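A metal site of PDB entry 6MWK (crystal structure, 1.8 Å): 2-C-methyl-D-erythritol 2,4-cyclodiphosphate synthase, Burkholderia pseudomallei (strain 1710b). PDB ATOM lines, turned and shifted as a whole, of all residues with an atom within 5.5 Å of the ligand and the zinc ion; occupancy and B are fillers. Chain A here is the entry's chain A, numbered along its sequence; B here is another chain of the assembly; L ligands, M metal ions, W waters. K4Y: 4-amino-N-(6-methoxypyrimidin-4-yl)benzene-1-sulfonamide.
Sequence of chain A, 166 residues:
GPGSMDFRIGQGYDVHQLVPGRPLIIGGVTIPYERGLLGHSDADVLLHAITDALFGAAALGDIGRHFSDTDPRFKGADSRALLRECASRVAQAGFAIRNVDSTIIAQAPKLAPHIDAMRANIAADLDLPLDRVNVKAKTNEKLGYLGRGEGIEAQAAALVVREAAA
NZ of Lys 138 of chain B is in hydrogen-bond range of N04 of the ligand (2.8 Å).
N16 of the ligand lies close to O of Phe 67, 3.1 Å away.
O11 of the ligand is in hydrogen-bond range of OG of Ser 41 (2.8 Å).
N of Ser 41 sits at hydrogen-bond distance from O11 of the ligand.
N of His 40 is in hydrogen-bond range of O11 of the ligand (3.1 Å).
A ring nitrogen (ND1) of His 16 sits at hydrogen-bond distance from the backbone carbonyl oxygen (O) of Leu 38, at 2.8 Å.
OD1 of Asp 69 lies within hydrogen-bond range of OG1 of Thr 70 (3.3 Å).
The side-chain hydroxyl (OG) of Ser 41 lies close to a ring nitrogen (NE2) of His 48 (3.3 Å).
OG of Ser 68 is in hydrogen-bond range of OG1 of Thr 70 (3.1 Å).
The backbone NH (N) of Ile 63 sits at hydrogen-bond distance from the side-chain carboxylate (OD1) of Asp 52, at 2.7 Å.
The side-chain hydroxyl of Ser 41 sits close to the backbone NH of Ala 43 (3.0 Å).
The side-chain carboxylate (OD2) of Asp 52 is in salt-bridge range of the side-chain amino group (NZ) of Lys 138 of chain B, at 2.8 Å.
Merely in contact with the ligand: Gly 39 (3.6 Å), Ile 63 (3.1 Å), Gly 64 (3.6 Å), Ser 68 (3.6 Å), Asp 69 (3.4 Å), Phe 74 (3.3 Å) and Leu 82 (3.6 Å).
Hydrophobic or aromatic side chains that line the ligand: His 16, His 40, His 48, Ile 63, Phe 67, Phe 74 and Leu 82.
Of the 25 residues printed, 14 come within 4 Å of the ligand.
Along chain A the residues within 4 Å of the ligand span positions 14 to 82.
The nearest printed residue that does not touch the ligand is Ala 43 (4.2 Å).
Within 4 Å of the zinc ion: Asp 14, His 16 and His 48.
The nearest printed residue that does not touch the zinc ion is Val 45 (4.7 Å).
The zinc ion is bound by N06 of the ligand (2.0 Å), ND1 of His 48 (2.0 Å), OD2 of Asp 14 (2.0 Å) and NE2 of His 16 (2.1 Å).
Slightly farther from the zinc ion lies N08 of the ligand (2.7 Å).
Water W2 lies within hydrogen-bond range of NZ of Lys 138 of chain B (2.5 Å), N of Gly 64 (2.9 Å) and O02 of the ligand (3.2 Å).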
ATOM      1  N   TYR A  13       2.358 -30.012   9.130  1.00  0.00           N
ATOM      2  CA  TYR A  13       1.296 -31.004   9.295  1.00  0.00           C
ATOM      3  C   TYR A  13      -0.039 -30.287   9.294  1.00  0.00           C
ATOM      4  O   TYR A  13      -0.165 -29.227   9.915  1.00  0.00           O
ATOM      5  CB  TYR A  13       1.449 -31.757  10.624  1.00  0.00           C
ATOM      6  CG  TYR A  13       0.227 -32.574  11.009  1.00  0.00           C
ATOM      7  CD1 TYR A  13       0.052 -33.847  10.486  1.00  0.00           C
ATOM      8  CD2 TYR A  13      -0.749 -32.077  11.860  1.00  0.00           C
ATOM      9  CE1 TYR A  13      -1.042 -34.609  10.823  1.00  0.00           C
ATOM     10  CE2 TYR A  13      -1.870 -32.838  12.184  1.00  0.00           C
ATOM     11  CZ  TYR A  13      -1.999 -34.111  11.668  1.00  0.00           C
ATOM     12  OH  TYR A  13      -3.098 -34.886  11.966  1.00  0.00           O
ATOM     13  N   ASP A  14      -1.049 -30.855   8.641  1.00  0.00           N
ATOM     14  CA  ASP A  14      -2.399 -30.338   8.828  1.00  0.00           C
ATOM     15  C   ASP A  14      -3.420 -31.447   8.601  1.00  0.00           C
ATOM     16  O   ASP A  14      -3.149 -32.417   7.900  1.00  0.00           O
ATOM     17  CB  ASP A  14      -2.652 -29.162   7.884  1.00  0.00           C
ATOM     18  CG  ASP A  14      -3.845 -28.336   8.300  1.00  0.00           C
ATOM     19  OD1 ASP A  14      -4.265 -28.402   9.471  1.00  0.00           O
ATOM     20  OD2 ASP A  14      -4.374 -27.605   7.446  1.00  0.00           O
ATOM     21  N   VAL A  15      -4.608 -31.267   9.169  1.00  0.00           N
ATOM     22  CA  VAL A  15      -5.732 -32.171   8.912  1.00  0.00           C
ATOM     23  C   VAL A  15      -7.018 -31.364   8.993  1.00  0.00           C
ATOM     24  O   VAL A  15      -7.132 -30.445   9.802  1.00  0.00           O
ATOM     25  CB  VAL A  15      -5.752 -33.369   9.901  1.00  0.00           C
ATOM     26  CG1 VAL A  15      -6.027 -32.893  11.337  1.00  0.00           C
ATOM     27  CG2 VAL A  15      -6.808 -34.399   9.472  1.00  0.00           C
ATOM     28  N   HIS A  16      -7.993 -31.719   8.149  1.00  0.00           N
ATOM     29  CA  HIS A  16      -9.328 -31.147   8.229  1.00  0.00           C
ATOM     30  C   HIS A  16     -10.347 -32.246   8.031  1.00  0.00           C
ATOM     31  O   HIS A  16     -10.114 -33.200   7.270  1.00  0.00           O
ATOM     32  CB  HIS A  16      -9.541 -30.057   7.155  1.00  0.00           C
ATOM     33  CG  HIS A  16      -8.836 -28.760   7.441  1.00  0.00           C
ATOM     34  ND1 HIS A  16      -9.479 -27.677   7.999  1.00  0.00           N
ATOM     35  CD2 HIS A  16      -7.556 -28.382   7.220  1.00  0.00           C
ATOM     36  CE1 HIS A  16      -8.613 -26.676   8.124  1.00  0.00           C
ATOM     37  NE2 HIS A  16      -7.453 -27.077   7.654  1.00  0.00           N
ATOM     38  N   LEU A  38     -13.662 -28.934   6.087  1.00  0.00           N
ATOM     39  CA  LEU A  38     -14.244 -27.983   7.029  1.00  0.00           C
ATOM     40  C   LEU A  38     -13.161 -27.124   7.675  1.00  0.00           C
ATOM     41  O   LEU A  38     -12.228 -27.656   8.283  1.00  0.00           O
ATOM     42  CB  LEU A  38     -15.017 -28.728   8.116  1.00  0.00           C
ATOM     43  CG  LEU A  38     -15.561 -27.863   9.238  1.00  0.00           C
ATOM     44  CD1 LEU A  38     -16.754 -27.074   8.730  1.00  0.00           C
ATOM     45  CD2 LEU A  38     -15.934 -28.737  10.428  1.00  0.00           C
ATOM     46  N   GLY A  39     -13.304 -25.806   7.570  1.00  0.00           N
ATOM     47  CA  GLY A  39     -12.371 -24.949   8.275  1.00  0.00           C
ATOM     48  C   GLY A  39     -12.859 -23.518   8.246  1.00  0.00           C
ATOM     49  O   GLY A  39     -13.823 -23.180   7.556  1.00  0.00           O
ATOM     50  N   HIS A  40     -12.178 -22.680   9.021  1.00  0.00           N
ATOM     51  CA  HIS A  40     -12.506 -21.253   9.013  1.00  0.00           C
ATOM     52  C   HIS A  40     -12.171 -20.642   7.656  1.00  0.00           C
ATOM     53  O   HIS A  40     -12.957 -19.857   7.108  1.00  0.00           O
ATOM     54  CB  HIS A  40     -11.750 -20.561  10.149  1.00  0.00           C
ATOM     55  CG  HIS A  40     -12.079 -19.105  10.300  1.00  0.00           C
ATOM     56  ND1 HIS A  40     -13.335 -18.652  10.626  1.00  0.00           N
ATOM     57  CD2 HIS A  40     -11.297 -18.001  10.164  1.00  0.00           C
ATOM     58  CE1 HIS A  40     -13.323 -17.325  10.686  1.00  0.00           C
ATOM     59  NE2 HIS A  40     -12.100 -16.911  10.415  1.00  0.00           N
ATOM     60  N   SER A  41     -11.021 -21.022   7.090  1.00  0.00           N
ATOM     61  CA  SER A  41     -10.595 -20.576   5.765  1.00  0.00           C
ATOM     62  C   SER A  41     -11.238 -21.464   4.709  1.00  0.00           C
ATOM     63  O   SER A  41     -12.208 -22.178   5.013  1.00  0.00           O
ATOM     64  CB  SER A  41      -9.076 -20.616   5.653  1.00  0.00           C
ATOM     65  OG  SER A  41      -8.581 -21.967   5.659  1.00  0.00           O
ATOM     66  N   ASP A  42     -10.715 -21.456   3.487  1.00  0.00           N
ATOM     67  CA  ASP A  42     -11.187 -22.457   2.536  1.00  0.00           C
ATOM     68  C   ASP A  42     -10.719 -23.868   2.907  1.00  0.00           C
ATOM     69  O   ASP A  42     -11.045 -24.831   2.182  1.00  0.00           O
ATOM     70  CB  ASP A  42     -10.746 -22.096   1.101  1.00  0.00           C
ATOM     71  CG  ASP A  42      -9.237 -22.128   0.887  1.00  0.00           C
ATOM     72  OD1 ASP A  42      -8.496 -22.655   1.738  1.00  0.00           O
ATOM     73  OD2 ASP A  42      -8.779 -21.674  -0.202  1.00  0.00           O
ATOM     74  N   ALA A  43      -9.961 -24.014   4.000  1.00  0.00           N
ATOM     75  CA  ALA A  43      -9.631 -25.310   4.586  1.00  0.00           C
ATOM     76  C   ALA A  43      -8.678 -26.136   3.725  1.00  0.00           C
ATOM     77  O   ALA A  43      -8.670 -27.381   3.807  1.00  0.00           O
ATOM     78  CB  ALA A  43     -10.896 -26.127   4.895  1.00  0.00           C
ATOM     79  N   ASP A  44      -7.841 -25.476   2.933  1.00  0.00           N
ATOM     80  CA  ASP A  44      -6.932 -26.156   2.020  1.00  0.00           C
ATOM     81  C   ASP A  44      -5.781 -26.816   2.789  1.00  0.00           C
ATOM     82  O   ASP A  44      -4.752 -26.188   3.080  1.00  0.00           O
ATOM     83  CB  ASP A  44      -6.396 -25.179   0.977  1.00  0.00           C
ATOM     84  CG  ASP A  44      -5.653 -25.864  -0.179  1.00  0.00           C
ATOM     85  OD1 ASP A  44      -4.978 -26.901   0.055  1.00  0.00           O
ATOM     86  OD2 ASP A  44      -5.717 -25.363  -1.315  1.00  0.00           O
ATOM     87  N   VAL A  45      -5.945 -28.099   3.102  1.00  0.00           N
ATOM     88  CA  VAL A  45      -5.054 -28.788   4.051  1.00  0.00           C
ATOM     89  C   VAL A  45      -3.609 -28.849   3.519  1.00  0.00           C
ATOM     90  O   VAL A  45      -2.649 -28.738   4.283  1.00  0.00           O
ATOM     91  CB  VAL A  45      -5.631 -30.176   4.370  1.00  0.00           C
ATOM     92  CG1 VAL A  45      -5.709 -31.046   3.135  1.00  0.00           C
ATOM     93  CG2 VAL A  45      -4.893 -30.894   5.494  1.00  0.00           C
ATOM     94  N   HIS A  48      -1.923 -25.385   3.819  1.00  0.00           N
ATOM     95  CA  HIS A  48      -1.638 -25.037   5.195  1.00  0.00           C
ATOM     96  C   HIS A  48      -0.404 -25.759   5.683  1.00  0.00           C
ATOM     97  O   HIS A  48       0.414 -25.189   6.398  1.00  0.00           O
ATOM     98  CB  HIS A  48      -2.814 -25.360   6.120  1.00  0.00           C
ATOM     99  CG  HIS A  48      -4.056 -24.584   5.808  1.00  0.00           C
ATOM    100  ND1 HIS A  48      -5.269 -24.834   6.420  1.00  0.00           N
ATOM    101  CD2 HIS A  48      -4.271 -23.553   4.953  1.00  0.00           C
ATOM    102  CE1 HIS A  48      -6.182 -24.010   5.940  1.00  0.00           C
ATOM    103  NE2 HIS A  48      -5.601 -23.209   5.054  1.00  0.00           N
ATOM    104  N   ASP A  52       2.997 -23.949   6.989  1.00  0.00           N
ATOM    105  CA  ASP A  52       3.637 -24.185   8.278  1.00  0.00           C
ATOM    106  C   ASP A  52       5.102 -24.602   8.097  1.00  0.00           C
ATOM    107  O   ASP A  52       5.961 -24.209   8.902  1.00  0.00           O
ATOM    108  CB  ASP A  52       2.873 -25.268   9.039  1.00  0.00           C
ATOM    109  CG  ASP A  52       2.015 -24.716  10.155  1.00  0.00           C
ATOM    110  OD1 ASP A  52       1.901 -23.474  10.264  1.00  0.00           O
ATOM    111  OD2 ASP A  52       1.478 -25.511  10.965  1.00  0.00           O
ATOM    112  N   ILE A  63       1.127 -20.998  11.151  1.00  0.00           N
ATOM    113  CA  ILE A  63       0.066 -20.318  10.419  1.00  0.00           C
ATOM    114  C   ILE A  63      -0.901 -19.661  11.398  1.00  0.00           C
ATOM    115  O   ILE A  63      -1.394 -18.549  11.144  1.00  0.00           O
ATOM    116  CB  ILE A  63      -0.597 -21.321   9.451  1.00  0.00           C
ATOM    117  CG1 ILE A  63      -1.488 -20.636   8.423  1.00  0.00           C
ATOM    118  CG2 ILE A  63      -1.363 -22.372  10.211  1.00  0.00           C
ATOM    119  CD1 ILE A  63      -2.089 -21.613   7.398  1.00  0.00           C
ATOM    120  N   GLY A  64      -1.116 -20.272  12.572  1.00  0.00           N
ATOM    121  CA  GLY A  64      -1.981 -19.671  13.579  1.00  0.00           C
ATOM    122  C   GLY A  64      -1.448 -18.366  14.133  1.00  0.00           C
ATOM    123  O   GLY A  64      -2.216 -17.469  14.460  1.00  0.00           O
ATOM    124  N   PHE A  67      -1.954 -15.845  10.863  1.00  0.00           N
ATOM    125  CA  PHE A  67      -3.295 -15.690  10.277  1.00  0.00           C
ATOM    126  C   PHE A  67      -4.294 -16.355  11.225  1.00  0.00           C
ATOM    127  O   PHE A  67      -4.594 -17.550  11.097  1.00  0.00           O
ATOM    128  CB  PHE A  67      -3.389 -16.312   8.892  1.00  0.00           C
ATOM    129  CG  PHE A  67      -2.253 -15.973   7.976  1.00  0.00           C
ATOM    130  CD1 PHE A  67      -2.055 -14.669   7.539  1.00  0.00           C
ATOM    131  CD2 PHE A  67      -1.399 -16.975   7.498  1.00  0.00           C
ATOM    132  CE1 PHE A  67      -1.021 -14.359   6.662  1.00  0.00           C
ATOM    133  CE2 PHE A  67      -0.356 -16.667   6.642  1.00  0.00           C
ATOM    134  CZ  PHE A  67      -0.178 -15.356   6.210  1.00  0.00           C
ATOM    135  N   SER A  68      -4.837 -15.573  12.151  1.00  0.00           N
ATOM    136  CA  SER A  68      -5.675 -16.111  13.225  1.00  0.00           C
ATOM    137  C   SER A  68      -6.892 -16.866  12.692  1.00  0.00           C
ATOM    138  O   SER A  68      -7.658 -16.351  11.855  1.00  0.00           O
ATOM    139  CB  SER A  68      -6.126 -14.979  14.148  1.00  0.00           C
ATOM    140  OG  SER A  68      -6.804 -15.501  15.269  1.00  0.00           O
ATOM    141  N   ASP A  69      -7.086 -18.080  13.206  1.00  0.00           N
ATOM    142  CA  ASP A  69      -8.239 -18.924  12.889  1.00  0.00           C
ATOM    143  C   ASP A  69      -9.558 -18.348  13.373  1.00  0.00           C
ATOM    144  O   ASP A  69     -10.612 -18.887  13.011  1.00  0.00           O
ATOM    145  CB  ASP A  69      -8.051 -20.314  13.509  1.00  0.00           C
ATOM    146  CG  ASP A  69      -7.661 -20.232  14.984  1.00  0.00           C
ATOM    147  OD1 ASP A  69      -7.841 -19.161  15.609  1.00  0.00           O
ATOM    148  OD2 ASP A  69      -7.166 -21.253  15.521  1.00  0.00           O
ATOM    149  N   THR A  70      -9.519 -17.316  14.203  1.00  0.00           N
ATOM    150  CA  THR A  70     -10.735 -16.690  14.708  1.00  0.00           C
ATOM    151  C   THR A  70     -10.914 -15.265  14.196  1.00  0.00           C
ATOM    152  O   THR A  70     -11.885 -14.599  14.567  1.00  0.00           O
ATOM    153  CB  THR A  70     -10.716 -16.689  16.244  1.00  0.00           C
ATOM    154  OG1 THR A  70      -9.391 -16.398  16.692  1.00  0.00           O
ATOM    155  CG2 THR A  70     -11.145 -18.045  16.768  1.00  0.00           C
ATOM    156  N   PHE A  74     -10.377 -13.672   7.807  1.00  0.00           N
ATOM    157  CA  PHE A  74      -9.925 -14.887   7.158  1.00  0.00           C
ATOM    158  C   PHE A  74     -11.041 -15.899   6.928  1.00  0.00           C
ATOM    159  O   PHE A  74     -10.752 -17.011   6.506  1.00  0.00           O
ATOM    160  CB  PHE A  74      -8.787 -15.519   7.955  1.00  0.00           C
ATOM    161  CG  PHE A  74      -7.582 -14.635   8.064  1.00  0.00           C
ATOM    162  CD1 PHE A  74      -6.913 -14.193   6.933  1.00  0.00           C
ATOM    163  CD2 PHE A  74      -7.105 -14.234   9.310  1.00  0.00           C
ATOM    164  CE1 PHE A  74      -5.807 -13.376   7.027  1.00  0.00           C
ATOM    165  CE2 PHE A  74      -5.996 -13.414   9.413  1.00  0.00           C
ATOM    166  CZ  PHE A  74      -5.352 -12.981   8.272  1.00  0.00           C
ATOM    167  N   ALA A  77     -11.008 -17.605   3.639  1.00  0.00           N
ATOM    168  CA  ALA A  77      -9.816 -17.069   3.001  1.00  0.00           C
ATOM    169  C   ALA A  77      -9.261 -18.019   1.943  1.00  0.00           C
ATOM    170  O   ALA A  77      -9.226 -19.242   2.143  1.00  0.00           O
ATOM    171  CB  ALA A  77      -8.725 -16.780   4.032  1.00  0.00           C
ATOM    172  N   LEU A  82      -2.904 -16.695   1.310  1.00  0.00           N
ATOM    173  CA  LEU A  82      -2.178 -16.839   2.563  1.00  0.00           C
ATOM    174  C   LEU A  82      -0.786 -17.427   2.331  1.00  0.00           C
ATOM    175  O   LEU A  82       0.192 -16.975   2.940  1.00  0.00           O
ATOM    176  CB  LEU A  82      -2.976 -17.730   3.512  1.00  0.00           C
ATOM    177  CG  LEU A  82      -4.331 -17.214   4.000  1.00  0.00           C
ATOM    178  CD1 LEU A  82      -4.933 -18.248   4.976  1.00  0.00           C
ATOM    179  CD2 LEU A  82      -4.265 -15.847   4.618  1.00  0.00           C
ATOM    180  N   LYS B 138      -0.723 -27.243  16.930  1.00  0.00           N
ATOM    181  CA  LYS B 138      -1.978 -27.434  16.175  1.00  0.00           C
ATOM    182  C   LYS B 138      -2.930 -28.303  16.991  1.00  0.00           C
ATOM    183  O   LYS B 138      -2.495 -29.063  17.848  1.00  0.00           O
ATOM    184  CB  LYS B 138      -1.755 -28.149  14.831  1.00  0.00           C
ATOM    185  CG  LYS B 138      -0.375 -28.020  14.202  1.00  0.00           C
ATOM    186  CD  LYS B 138      -0.114 -26.616  13.701  1.00  0.00           C
ATOM    187  CE  LYS B 138      -1.124 -26.198  12.653  1.00  0.00           C
ATOM    188  NZ  LYS B 138      -0.881 -24.763  12.296  1.00  0.00           N
ATOM    189  N   GLU B 141      -8.314 -31.180  14.873  1.00  0.00           N
ATOM    190  CA  GLU B 141      -9.661 -30.971  14.359  1.00  0.00           C
ATOM    191  C   GLU B 141     -10.637 -32.047  14.845  1.00  0.00           C
ATOM    192  O   GLU B 141     -11.512 -32.504  14.118  1.00  0.00           O
ATOM    193  CB  GLU B 141      -9.651 -30.879  12.832  1.00  0.00           C
ATOM    194  CG  GLU B 141      -9.049 -29.579  12.321  1.00  0.00           C
ATOM    195  CD  GLU B 141      -9.892 -28.377  12.680  1.00  0.00           C
ATOM    196  OE1 GLU B 141     -11.087 -28.368  12.314  1.00  0.00           O
ATOM    197  OE2 GLU B 141      -9.382 -27.461  13.342  1.00  0.00           O
HETATM  198  C01 K4Y L   1      -4.807 -21.826  13.126  1.00  0.00           C
HETATM  199  C03 K4Y L   1      -4.274 -23.587  11.554  1.00  0.00           C
HETATM  200  C05 K4Y L   1      -3.737 -25.160   9.998  1.00  0.00           C
HETATM  201  C07 K4Y L   1      -5.727 -24.099   9.791  1.00  0.00           C
HETATM  202  C12 K4Y L   1      -7.486 -21.348   9.061  1.00  0.00           C
HETATM  203  C13 K4Y L   1      -8.146 -20.264   9.603  1.00  0.00           C
HETATM  204  C14 K4Y L   1      -7.666 -19.000   9.394  1.00  0.00           C
HETATM  205  C15 K4Y L   1      -6.529 -18.799   8.613  1.00  0.00           C
HETATM  206  C17 K4Y L   1      -5.885 -19.913   8.055  1.00  0.00           C
HETATM  207  C18 K4Y L   1      -6.372 -21.187   8.271  1.00  0.00           C
HETATM  208  C19 K4Y L   1      -5.481 -23.337  10.913  1.00  0.00           C
HETATM  209  N04 K4Y L   1      -3.418 -24.497  11.097  1.00  0.00           N
HETATM  210  N06 K4Y L   1      -4.866 -25.015   9.345  1.00  0.00           N
HETATM  211  N08 K4Y L   1      -6.856 -23.989   9.027  1.00  0.00           N
HETATM  212  N16 K4Y L   1      -6.057 -17.545   8.411  1.00  0.00           N
HETATM  213  O02 K4Y L   1      -3.945 -22.901  12.652  1.00  0.00           O
HETATM  214  O10 K4Y L   1      -8.692 -23.052  10.813  1.00  0.00           O
HETATM  215  O11 K4Y L   1      -9.214 -23.152   8.126  1.00  0.00           O
HETATM  216  S09 K4Y L   1      -8.203 -22.957   9.317  1.00  0.00           S
HETATM  217 ZN    ZN M   1      -5.657 -26.114   7.893  1.00  0.00          ZN
HETATM  218  O   HOH W   1      -0.949 -26.467   9.183  1.00  0.00           O
HETATM  219  O   HOH W   2      -0.999 -22.821  13.933  1.00  0.00           O
